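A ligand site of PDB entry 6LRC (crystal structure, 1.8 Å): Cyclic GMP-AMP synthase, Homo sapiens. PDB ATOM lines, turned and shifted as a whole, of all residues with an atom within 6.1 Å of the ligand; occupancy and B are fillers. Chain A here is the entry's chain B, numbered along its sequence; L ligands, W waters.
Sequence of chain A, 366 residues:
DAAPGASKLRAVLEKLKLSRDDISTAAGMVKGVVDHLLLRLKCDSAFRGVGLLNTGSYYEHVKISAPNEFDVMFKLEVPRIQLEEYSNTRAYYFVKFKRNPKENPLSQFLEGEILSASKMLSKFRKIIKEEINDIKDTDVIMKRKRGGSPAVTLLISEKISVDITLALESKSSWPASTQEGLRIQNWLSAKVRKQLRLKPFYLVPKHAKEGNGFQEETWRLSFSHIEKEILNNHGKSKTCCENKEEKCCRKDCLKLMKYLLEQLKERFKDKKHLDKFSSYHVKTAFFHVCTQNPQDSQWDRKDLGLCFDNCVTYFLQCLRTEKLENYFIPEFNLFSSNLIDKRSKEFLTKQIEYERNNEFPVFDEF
The side-chain amino group (NZ) of Lys 206 lies within salt-bridge range of an oxygen (O2) of the ligand (3.5 Å).
The side-chain hydroxyl (OG) of Ser 278 is in hydrogen-bond range of an oxygen (O4) of the ligand, at 3.1 Å.
NH1 of Arg 220 is in salt-bridge range of O2 of the ligand, at 2.9 Å.
O of Ser 149 lies within hydrogen-bond range of NZ of Lys 206 (2.6 Å).
N of Tyr 280 lies close to OG of Ser 278 (3.0 Å).
The side-chain amide oxygen of Asn 326 is in hydrogen-bond range of the backbone NH of Ile 329.
The side-chain hydroxyl (OG) of Ser 224 sits at hydrogen-bond distance from the side-chain hydroxyl (OG) of Ser 222, at 3.1 Å.
The backbone carbonyl oxygen (O) of Arg 146 sits at hydrogen-bond distance from the side-chain amino group (NZ) of Lys 206 (2.9 Å).
ND1 of His 281 sits at hydrogen-bond distance from N of Ser 278.
N of Leu 221 is in hydrogen-bond range of O of Ala 91 (3.0 Å).
OH of Tyr 92 is in hydrogen-bond range of NH1 of Arg 220 (3.2 Å).
Ala 91 touches the ligand.
Leu 221 touches the ligand (O to C1, 3.6 Å).
Ser 224 touches the ligand.
Tyr 280 touches the ligand.
NE2 of His 281 touches C3 of the ligand, 3.5 Å away.
ND2 of Asn 326 touches C15 of the ligand, at 3.5 Å.
CE1 of Phe 332 touches C13 of the ligand, 3.4 Å away.
CD2 of Leu 334 touches C13 of the ligand, at 3.6 Å.
Hydrophobic or aromatic side chains within 4 Å of the ligand: Ala 91, Tyr 280, His 281, Phe 332 and Leu 334.
Of the 21 residues printed, 11 come within 4 Å of the ligand.
The nearest printed residue that does not touch the ligand is Ser 222 (4.01 Å).
Water W6 lies within hydrogen-bond range of OG of Ser 222, O1 of the ligand and OG of Ser 224.
Water W4 lies within hydrogen-bond range of an oxygen (O3) of the ligand (2.6 Å), the side-chain amino group of Lys 206 (2.6 Å) and the guanidinium group of Arg 146 (2.8 Å).
Water W2 lies within hydrogen-bond range of an oxygen (O1) of the ligand (2.7 Å), the side-chain carboxylate of Glu 227 (2.8 Å), the backbone NH of Phe 223 (2.8 Å) and the side-chain hydroxyl of Tyr 280 (3.4 Å).
Water W1 lies within hydrogen-bond range of OE2 of Glu 227, O1 of the ligand and OG of Ser 224.
Water W3 lies within hydrogen-bond range of a ring nitrogen (NE2) of His 281 (2.7 Å) and the backbone carbonyl oxygen (O) of Leu 334 (2.8 Å).
Water W5 lies within hydrogen-bond range of ND2 of Asn 326 and O of Leu 221.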
ATOM      1  N   ALA A  91       2.082  -4.459 -22.017  1.00  0.00           N
ATOM      2  CA  ALA A  91       1.329  -3.246 -22.306  1.00  0.00           C
ATOM      3  C   ALA A  91       1.618  -2.072 -21.367  1.00  0.00           C
ATOM      4  O   ALA A  91       1.301  -0.932 -21.739  1.00  0.00           O
ATOM      5  CB  ALA A  91      -0.182  -3.522 -22.253  1.00  0.00           C
ATOM      6  N   TYR A  92       2.182  -2.308 -20.184  1.00  0.00           N
ATOM      7  CA  TYR A  92       2.428  -1.266 -19.202  1.00  0.00           C
ATOM      8  C   TYR A  92       3.917  -1.017 -19.057  1.00  0.00           C
ATOM      9  O   TYR A  92       4.720  -1.950 -19.054  1.00  0.00           O
ATOM     10  CB  TYR A  92       1.856  -1.636 -17.822  1.00  0.00           C
ATOM     11  CG  TYR A  92       0.344  -1.775 -17.810  1.00  0.00           C
ATOM     12  CD1 TYR A  92      -0.259  -2.954 -18.242  1.00  0.00           C
ATOM     13  CD2 TYR A  92      -0.467  -0.741 -17.352  1.00  0.00           C
ATOM     14  CE1 TYR A  92      -1.649  -3.084 -18.230  1.00  0.00           C
ATOM     15  CE2 TYR A  92      -1.849  -0.866 -17.342  1.00  0.00           C
ATOM     16  CZ  TYR A  92      -2.438  -2.045 -17.772  1.00  0.00           C
ATOM     17  OH  TYR A  92      -3.814  -2.177 -17.759  1.00  0.00           O
ATOM     18  N   ARG A 146     -10.203   4.603 -12.468  1.00  0.00           N
ATOM     19  CA  ARG A 146      -9.815   4.224 -13.819  1.00  0.00           C
ATOM     20  C   ARG A 146      -8.301   4.282 -13.982  1.00  0.00           C
ATOM     21  O   ARG A 146      -7.814   4.387 -15.120  1.00  0.00           O
ATOM     22  CB  ARG A 146     -10.496   5.096 -14.872  1.00  0.00           C
ATOM     23  CG  ARG A 146     -12.017   5.014 -14.875  1.00  0.00           C
ATOM     24  CD  ARG A 146     -12.518   3.682 -15.381  1.00  0.00           C
ATOM     25  NE  ARG A 146     -12.243   3.510 -16.804  1.00  0.00           N
ATOM     26  CZ  ARG A 146     -12.954   4.100 -17.767  1.00  0.00           C
ATOM     27  NH1 ARG A 146     -13.981   4.887 -17.454  1.00  0.00           N
ATOM     28  NH2 ARG A 146     -12.645   3.897 -19.040  1.00  0.00           N
ATOM     29  N   SER A 149      -6.786   7.177 -16.377  1.00  0.00           N
ATOM     30  CA  SER A 149      -7.232   7.400 -17.751  1.00  0.00           C
ATOM     31  C   SER A 149      -8.618   6.798 -17.913  1.00  0.00           C
ATOM     32  O   SER A 149      -8.758   5.556 -17.846  1.00  0.00           O
ATOM     33  CB  SER A 149      -6.261   6.787 -18.766  1.00  0.00           C
ATOM     34  OG  SER A 149      -4.985   7.429 -18.722  1.00  0.00           O
ATOM     35  N   LYS A 206      -1.833   4.867 -16.466  1.00  0.00           N
ATOM     36  CA  LYS A 206      -2.712   3.747 -16.128  1.00  0.00           C
ATOM     37  C   LYS A 206      -2.022   2.876 -15.086  1.00  0.00           C
ATOM     38  O   LYS A 206      -1.023   2.208 -15.400  1.00  0.00           O
ATOM     39  CB  LYS A 206      -3.055   2.946 -17.384  1.00  0.00           C
ATOM     40  CG  LYS A 206      -4.362   2.178 -17.264  1.00  0.00           C
ATOM     41  CD  LYS A 206      -5.582   3.089 -17.414  1.00  0.00           C
ATOM     42  CE  LYS A 206      -6.892   2.277 -17.341  1.00  0.00           C
ATOM     43  NZ  LYS A 206      -8.094   3.084 -17.708  1.00  0.00           N
ATOM     44  N   ARG A 220       0.253   2.949 -20.173  1.00  0.00           N
ATOM     45  CA  ARG A 220      -0.195   1.861 -21.013  1.00  0.00           C
ATOM     46  C   ARG A 220      -0.223   2.266 -22.477  1.00  0.00           C
ATOM     47  O   ARG A 220      -0.618   3.385 -22.814  1.00  0.00           O
ATOM     48  CB  ARG A 220      -1.586   1.383 -20.570  1.00  0.00           C
ATOM     49  CG  ARG A 220      -2.014   0.112 -21.272  1.00  0.00           C
ATOM     50  CD  ARG A 220      -3.320  -0.381 -20.680  1.00  0.00           C
ATOM     51  NE  ARG A 220      -4.448   0.456 -21.063  1.00  0.00           N
ATOM     52  CZ  ARG A 220      -5.670   0.305 -20.571  1.00  0.00           C
ATOM     53  NH1 ARG A 220      -5.903  -0.645 -19.664  1.00  0.00           N
ATOM     54  NH2 ARG A 220      -6.653   1.101 -20.974  1.00  0.00           N
ATOM     55  N   LEU A 221       0.181   1.348 -23.352  1.00  0.00           N
ATOM     56  CA  LEU A 221       0.241   1.633 -24.785  1.00  0.00           C
ATOM     57  C   LEU A 221      -1.156   1.871 -25.336  1.00  0.00           C
ATOM     58  O   LEU A 221      -2.104   1.174 -24.987  1.00  0.00           O
ATOM     59  CB  LEU A 221       0.885   0.475 -25.536  1.00  0.00           C
ATOM     60  CG  LEU A 221       2.364   0.245 -25.265  1.00  0.00           C
ATOM     61  CD1 LEU A 221       2.884  -0.984 -26.021  1.00  0.00           C
ATOM     62  CD2 LEU A 221       3.130   1.493 -25.662  1.00  0.00           C
ATOM     63  N   SER A 222      -1.260   2.866 -26.214  1.00  0.00           N
ATOM     64  CA  SER A 222      -2.507   3.231 -26.860  1.00  0.00           C
ATOM     65  C   SER A 222      -2.244   3.455 -28.342  1.00  0.00           C
ATOM     66  O   SER A 222      -1.285   4.128 -28.723  1.00  0.00           O
ATOM     67  CB  SER A 222      -3.119   4.504 -26.245  1.00  0.00           C
ATOM     68  OG  SER A 222      -4.237   4.893 -27.031  1.00  0.00           O
ATOM     69  N   PHE A 223      -3.111   2.892 -29.179  1.00  0.00           N
ATOM     70  CA  PHE A 223      -3.009   3.019 -30.624  1.00  0.00           C
ATOM     71  C   PHE A 223      -4.339   3.499 -31.188  1.00  0.00           C
ATOM     72  O   PHE A 223      -4.748   3.084 -32.272  1.00  0.00           O
ATOM     73  CB  PHE A 223      -2.572   1.687 -31.244  1.00  0.00           C
ATOM     74  CG  PHE A 223      -1.230   1.217 -30.760  1.00  0.00           C
ATOM     75  CD1 PHE A 223      -0.059   1.661 -31.377  1.00  0.00           C
ATOM     76  CD2 PHE A 223      -1.117   0.356 -29.677  1.00  0.00           C
ATOM     77  CE1 PHE A 223       1.203   1.239 -30.912  1.00  0.00           C
ATOM     78  CE2 PHE A 223       0.125  -0.080 -29.230  1.00  0.00           C
ATOM     79  CZ  PHE A 223       1.289   0.375 -29.843  1.00  0.00           C
ATOM     80  N   SER A 224      -5.041   4.378 -30.450  1.00  0.00           N
ATOM     81  CA  SER A 224      -6.391   4.763 -30.864  1.00  0.00           C
ATOM     82  C   SER A 224      -6.403   5.443 -32.229  1.00  0.00           C
ATOM     83  O   SER A 224      -7.407   5.373 -32.951  1.00  0.00           O
ATOM     84  CB  SER A 224      -7.026   5.683 -29.818  1.00  0.00           C
ATOM     85  OG  SER A 224      -6.904   5.121 -28.527  1.00  0.00           O
ATOM     86  N   GLU A 227      -6.423   2.611 -34.817  1.00  0.00           N
ATOM     87  CA  GLU A 227      -7.750   1.991 -34.898  1.00  0.00           C
ATOM     88  C   GLU A 227      -8.694   2.862 -35.705  1.00  0.00           C
ATOM     89  O   GLU A 227      -9.499   2.361 -36.508  1.00  0.00           O
ATOM     90  CB  GLU A 227      -8.298   1.765 -33.481  1.00  0.00           C
ATOM     91  CG  GLU A 227      -7.359   0.876 -32.645  1.00  0.00           C
ATOM     92  CD  GLU A 227      -7.683   0.886 -31.144  1.00  0.00           C
ATOM     93  OE1 GLU A 227      -6.945   0.242 -30.352  1.00  0.00           O
ATOM     94  OE2 GLU A 227      -8.671   1.549 -30.749  1.00  0.00           O
ATOM     95  N   LYS A 276     -17.584  -5.602 -16.326  1.00  0.00           N
ATOM     96  CA  LYS A 276     -16.188  -5.623 -16.754  1.00  0.00           C
ATOM     97  C   LYS A 276     -16.020  -5.653 -18.275  1.00  0.00           C
ATOM     98  O   LYS A 276     -14.898  -5.488 -18.762  1.00  0.00           O
ATOM     99  CB  LYS A 276     -15.460  -6.800 -16.121  1.00  0.00           C
ATOM    100  CG  LYS A 276     -15.079  -6.580 -14.656  1.00  0.00           C
ATOM    101  CD  LYS A 276     -14.312  -7.762 -14.093  1.00  0.00           C
ATOM    102  CE  LYS A 276     -15.194  -9.000 -13.990  1.00  0.00           C
ATOM    103  NZ  LYS A 276     -14.515 -10.125 -13.287  1.00  0.00           N
ATOM    104  N   SER A 278     -16.494  -4.194 -22.147  1.00  0.00           N
ATOM    105  CA  SER A 278     -16.551  -2.864 -22.706  1.00  0.00           C
ATOM    106  C   SER A 278     -16.537  -2.927 -24.219  1.00  0.00           C
ATOM    107  O   SER A 278     -16.239  -3.964 -24.844  1.00  0.00           O
ATOM    108  CB  SER A 278     -15.401  -1.994 -22.173  1.00  0.00           C
ATOM    109  OG  SER A 278     -14.336  -1.948 -23.076  1.00  0.00           O
ATOM    110  N   SER A 279     -16.906  -1.789 -24.827  1.00  0.00           N
ATOM    111  CA  SER A 279     -16.876  -1.671 -26.276  1.00  0.00           C
ATOM    112  C   SER A 279     -15.525  -2.057 -26.843  1.00  0.00           C
ATOM    113  O   SER A 279     -15.457  -2.522 -27.982  1.00  0.00           O
ATOM    114  CB  SER A 279     -17.209  -0.229 -26.708  1.00  0.00           C
ATOM    115  OG  SER A 279     -16.223   0.673 -26.219  1.00  0.00           O
ATOM    116  N   TYR A 280     -14.446  -1.856 -26.083  1.00  0.00           N
ATOM    117  CA  TYR A 280     -13.128  -2.202 -26.605  1.00  0.00           C
ATOM    118  C   TYR A 280     -12.994  -3.698 -26.866  1.00  0.00           C
ATOM    119  O   TYR A 280     -12.248  -4.119 -27.771  1.00  0.00           O
ATOM    120  CB  TYR A 280     -12.023  -1.728 -25.657  1.00  0.00           C
ATOM    121  CG  TYR A 280     -10.676  -1.730 -26.341  1.00  0.00           C
ATOM    122  CD1 TYR A 280     -10.435  -0.847 -27.382  1.00  0.00           C
ATOM    123  CD2 TYR A 280      -9.682  -2.646 -26.015  1.00  0.00           C
ATOM    124  CE1 TYR A 280      -9.225  -0.835 -28.055  1.00  0.00           C
ATOM    125  CE2 TYR A 280      -8.455  -2.643 -26.704  1.00  0.00           C
ATOM    126  CZ  TYR A 280      -8.236  -1.727 -27.730  1.00  0.00           C
ATOM    127  OH  TYR A 280      -7.042  -1.686 -28.428  1.00  0.00           O
ATOM    128  N   HIS A 281     -13.683  -4.528 -26.075  1.00  0.00           N
ATOM    129  CA  HIS A 281     -13.650  -5.984 -26.311  1.00  0.00           C
ATOM    130  C   HIS A 281     -14.291  -6.327 -27.651  1.00  0.00           C
ATOM    131  O   HIS A 281     -13.710  -7.085 -28.446  1.00  0.00           O
ATOM    132  CB  HIS A 281     -14.354  -6.720 -25.167  1.00  0.00           C
ATOM    133  CG  HIS A 281     -13.658  -6.608 -23.860  1.00  0.00           C
ATOM    134  ND1 HIS A 281     -14.280  -6.111 -22.732  1.00  0.00           N
ATOM    135  CD2 HIS A 281     -12.407  -6.942 -23.481  1.00  0.00           C
ATOM    136  CE1 HIS A 281     -13.435  -6.131 -21.724  1.00  0.00           C
ATOM    137  NE2 HIS A 281     -12.282  -6.616 -22.147  1.00  0.00           N
ATOM    138  N   ASN A 326      -5.151  -8.383 -27.444  1.00  0.00           N
ATOM    139  CA  ASN A 326      -5.001  -7.018 -27.941  1.00  0.00           C
ATOM    140  C   ASN A 326      -4.492  -7.034 -29.386  1.00  0.00           C
ATOM    141  O   ASN A 326      -3.564  -7.769 -29.733  1.00  0.00           O
ATOM    142  CB  ASN A 326      -4.042  -6.264 -27.014  1.00  0.00           C
ATOM    143  CG  ASN A 326      -3.880  -4.816 -27.403  1.00  0.00           C
ATOM    144  OD1 ASN A 326      -3.342  -4.521 -28.466  1.00  0.00           O
ATOM    145  ND2 ASN A 326      -4.353  -3.898 -26.547  1.00  0.00           N
ATOM    146  N   ILE A 329      -0.899  -5.868 -29.425  1.00  0.00           N
ATOM    147  CA  ILE A 329       0.017  -6.510 -28.471  1.00  0.00           C
ATOM    148  C   ILE A 329      -0.446  -7.944 -28.276  1.00  0.00           C
ATOM    149  O   ILE A 329      -1.203  -8.243 -27.335  1.00  0.00           O
ATOM    150  CB  ILE A 329       0.052  -5.748 -27.123  1.00  0.00           C
ATOM    151  CG1 ILE A 329       0.165  -4.234 -27.338  1.00  0.00           C
ATOM    152  CG2 ILE A 329       1.128  -6.347 -26.170  1.00  0.00           C
ATOM    153  CD1 ILE A 329      -0.350  -3.380 -26.160  1.00  0.00           C
ATOM    154  N   PHE A 332      -0.941  -9.897 -24.844  1.00  0.00           N
ATOM    155  CA  PHE A 332      -1.827  -9.373 -23.813  1.00  0.00           C
ATOM    156  C   PHE A 332      -3.222  -9.895 -24.078  1.00  0.00           C
ATOM    157  O   PHE A 332      -3.878  -9.494 -25.049  1.00  0.00           O
ATOM    158  CB  PHE A 332      -1.806  -7.848 -23.779  1.00  0.00           C
ATOM    159  CG  PHE A 332      -2.412  -7.267 -22.522  1.00  0.00           C
ATOM    160  CD1 PHE A 332      -3.789  -7.203 -22.365  1.00  0.00           C
ATOM    161  CD2 PHE A 332      -1.599  -6.806 -21.490  1.00  0.00           C
ATOM    162  CE1 PHE A 332      -4.341  -6.694 -21.223  1.00  0.00           C
ATOM    163  CE2 PHE A 332      -2.152  -6.293 -20.340  1.00  0.00           C
ATOM    164  CZ  PHE A 332      -3.525  -6.225 -20.206  1.00  0.00           C
ATOM    165  N   LEU A 334      -6.896  -9.836 -23.353  1.00  0.00           N
ATOM    166  CA  LEU A 334      -7.971  -9.069 -22.706  1.00  0.00           C
ATOM    167  C   LEU A 334      -8.932  -9.973 -21.946  1.00  0.00           C
ATOM    168  O   LEU A 334      -9.614  -9.510 -21.019  1.00  0.00           O
ATOM    169  CB  LEU A 334      -8.790  -8.275 -23.728  1.00  0.00           C
ATOM    170  CG  LEU A 334      -7.997  -7.355 -24.658  1.00  0.00           C
ATOM    171  CD1 LEU A 334      -8.930  -6.663 -25.625  1.00  0.00           C
ATOM    172  CD2 LEU A 334      -7.206  -6.340 -23.855  1.00  0.00           C
ATOM    173  N   LEU A 339      -8.453 -10.612 -15.566  1.00  0.00           N
ATOM    174  CA  LEU A 339      -9.215  -9.418 -15.902  1.00  0.00           C
ATOM    175  C   LEU A 339     -10.715  -9.646 -15.859  1.00  0.00           C
ATOM    176  O   LEU A 339     -11.467  -8.742 -15.524  1.00  0.00           O
ATOM    177  CB  LEU A 339      -8.827  -8.932 -17.299  1.00  0.00           C
ATOM    178  CG  LEU A 339      -7.353  -8.535 -17.388  1.00  0.00           C
ATOM    179  CD1 LEU A 339      -6.977  -8.052 -18.796  1.00  0.00           C
ATOM    180  CD2 LEU A 339      -7.052  -7.436 -16.315  1.00  0.00           C
HETATM  181  C1  LIG L   1      -4.351  -1.433 -24.039  1.00  0.00           C
HETATM  182  C2  LIG L   1     -10.124   0.494 -23.772  1.00  0.00           C
HETATM  183  C3  LIG L   1     -11.036  -3.418 -21.513  1.00  0.00           C
HETATM  184  C4  LIG L   1      -8.618  -2.647 -20.021  1.00  0.00           C
HETATM  185  C5  LIG L   1      -9.971  -1.955 -19.768  1.00  0.00           C
HETATM  186  C6  LIG L   1      -9.793  -0.541 -19.215  1.00  0.00           C
HETATM  187  C7  LIG L   1     -10.556   1.568 -24.579  1.00  0.00           C
HETATM  188  O1  LIG L   1      -7.046   2.055 -26.714  1.00  0.00           O
HETATM  189  C8  LIG L   1      -7.316   1.181 -25.768  1.00  0.00           C
HETATM  190  C9  LIG L   1      -6.372   0.242 -25.295  1.00  0.00           C
HETATM  191  C10 LIG L   1      -6.704  -0.664 -24.276  1.00  0.00           C
HETATM  192  C11 LIG L   1      -5.706  -1.636 -23.792  1.00  0.00           C
HETATM  193  C12 LIG L   1      -6.093  -2.764 -23.087  1.00  0.00           C
HETATM  194  C13 LIG L   1      -5.144  -3.669 -22.639  1.00  0.00           C
HETATM  195  C14 LIG L   1      -3.808  -3.458 -22.891  1.00  0.00           C
HETATM  196  C15 LIG L   1      -3.409  -2.343 -23.589  1.00  0.00           C
HETATM  197  N1  LIG L   1      -7.938  -0.670 -23.685  1.00  0.00           N
HETATM  198  C16 LIG L   1      -8.805   0.254 -24.154  1.00  0.00           C
HETATM  199  C17 LIG L   1     -10.897  -0.202 -22.732  1.00  0.00           C
HETATM  200  N2  LIG L   1     -10.229  -1.184 -22.094  1.00  0.00           N
HETATM  201  C18 LIG L   1     -10.848  -1.989 -21.031  1.00  0.00           C
HETATM  202  C19 LIG L   1      -9.677  -4.037 -21.831  1.00  0.00           C
HETATM  203  C20 LIG L   1      -8.793  -4.052 -20.588  1.00  0.00           C
HETATM  204  O2  LIG L   1      -8.665  -0.106 -19.117  1.00  0.00           O
HETATM  205  O3  LIG L   1     -10.778   0.088 -18.915  1.00  0.00           O
HETATM  206  O4  LIG L   1     -12.068   0.109 -22.464  1.00  0.00           O
HETATM  207  N3  LIG L   1      -8.541   1.156 -25.147  1.00  0.00           N
HETATM  208  N4  LIG L   1      -9.606   1.964 -25.421  1.00  0.00           N
HETATM  209  O   HOH W   1      -9.125   2.890 -28.471  1.00  0.00           O
HETATM  210  O   HOH W   2      -5.200   1.168 -28.421  1.00  0.00           O
HETATM  211  O   HOH W   3     -10.304  -6.874 -20.286  1.00  0.00           O
HETATM  212  O   HOH W   4     -10.142   1.648 -16.920  1.00  0.00           O
HETATM  213  O   HOH W   5      -3.671  -0.831 -27.262  1.00  0.00           O
HETATM  214  O   HOH W   6      -6.316   4.305 -25.658  1.00  0.00           O
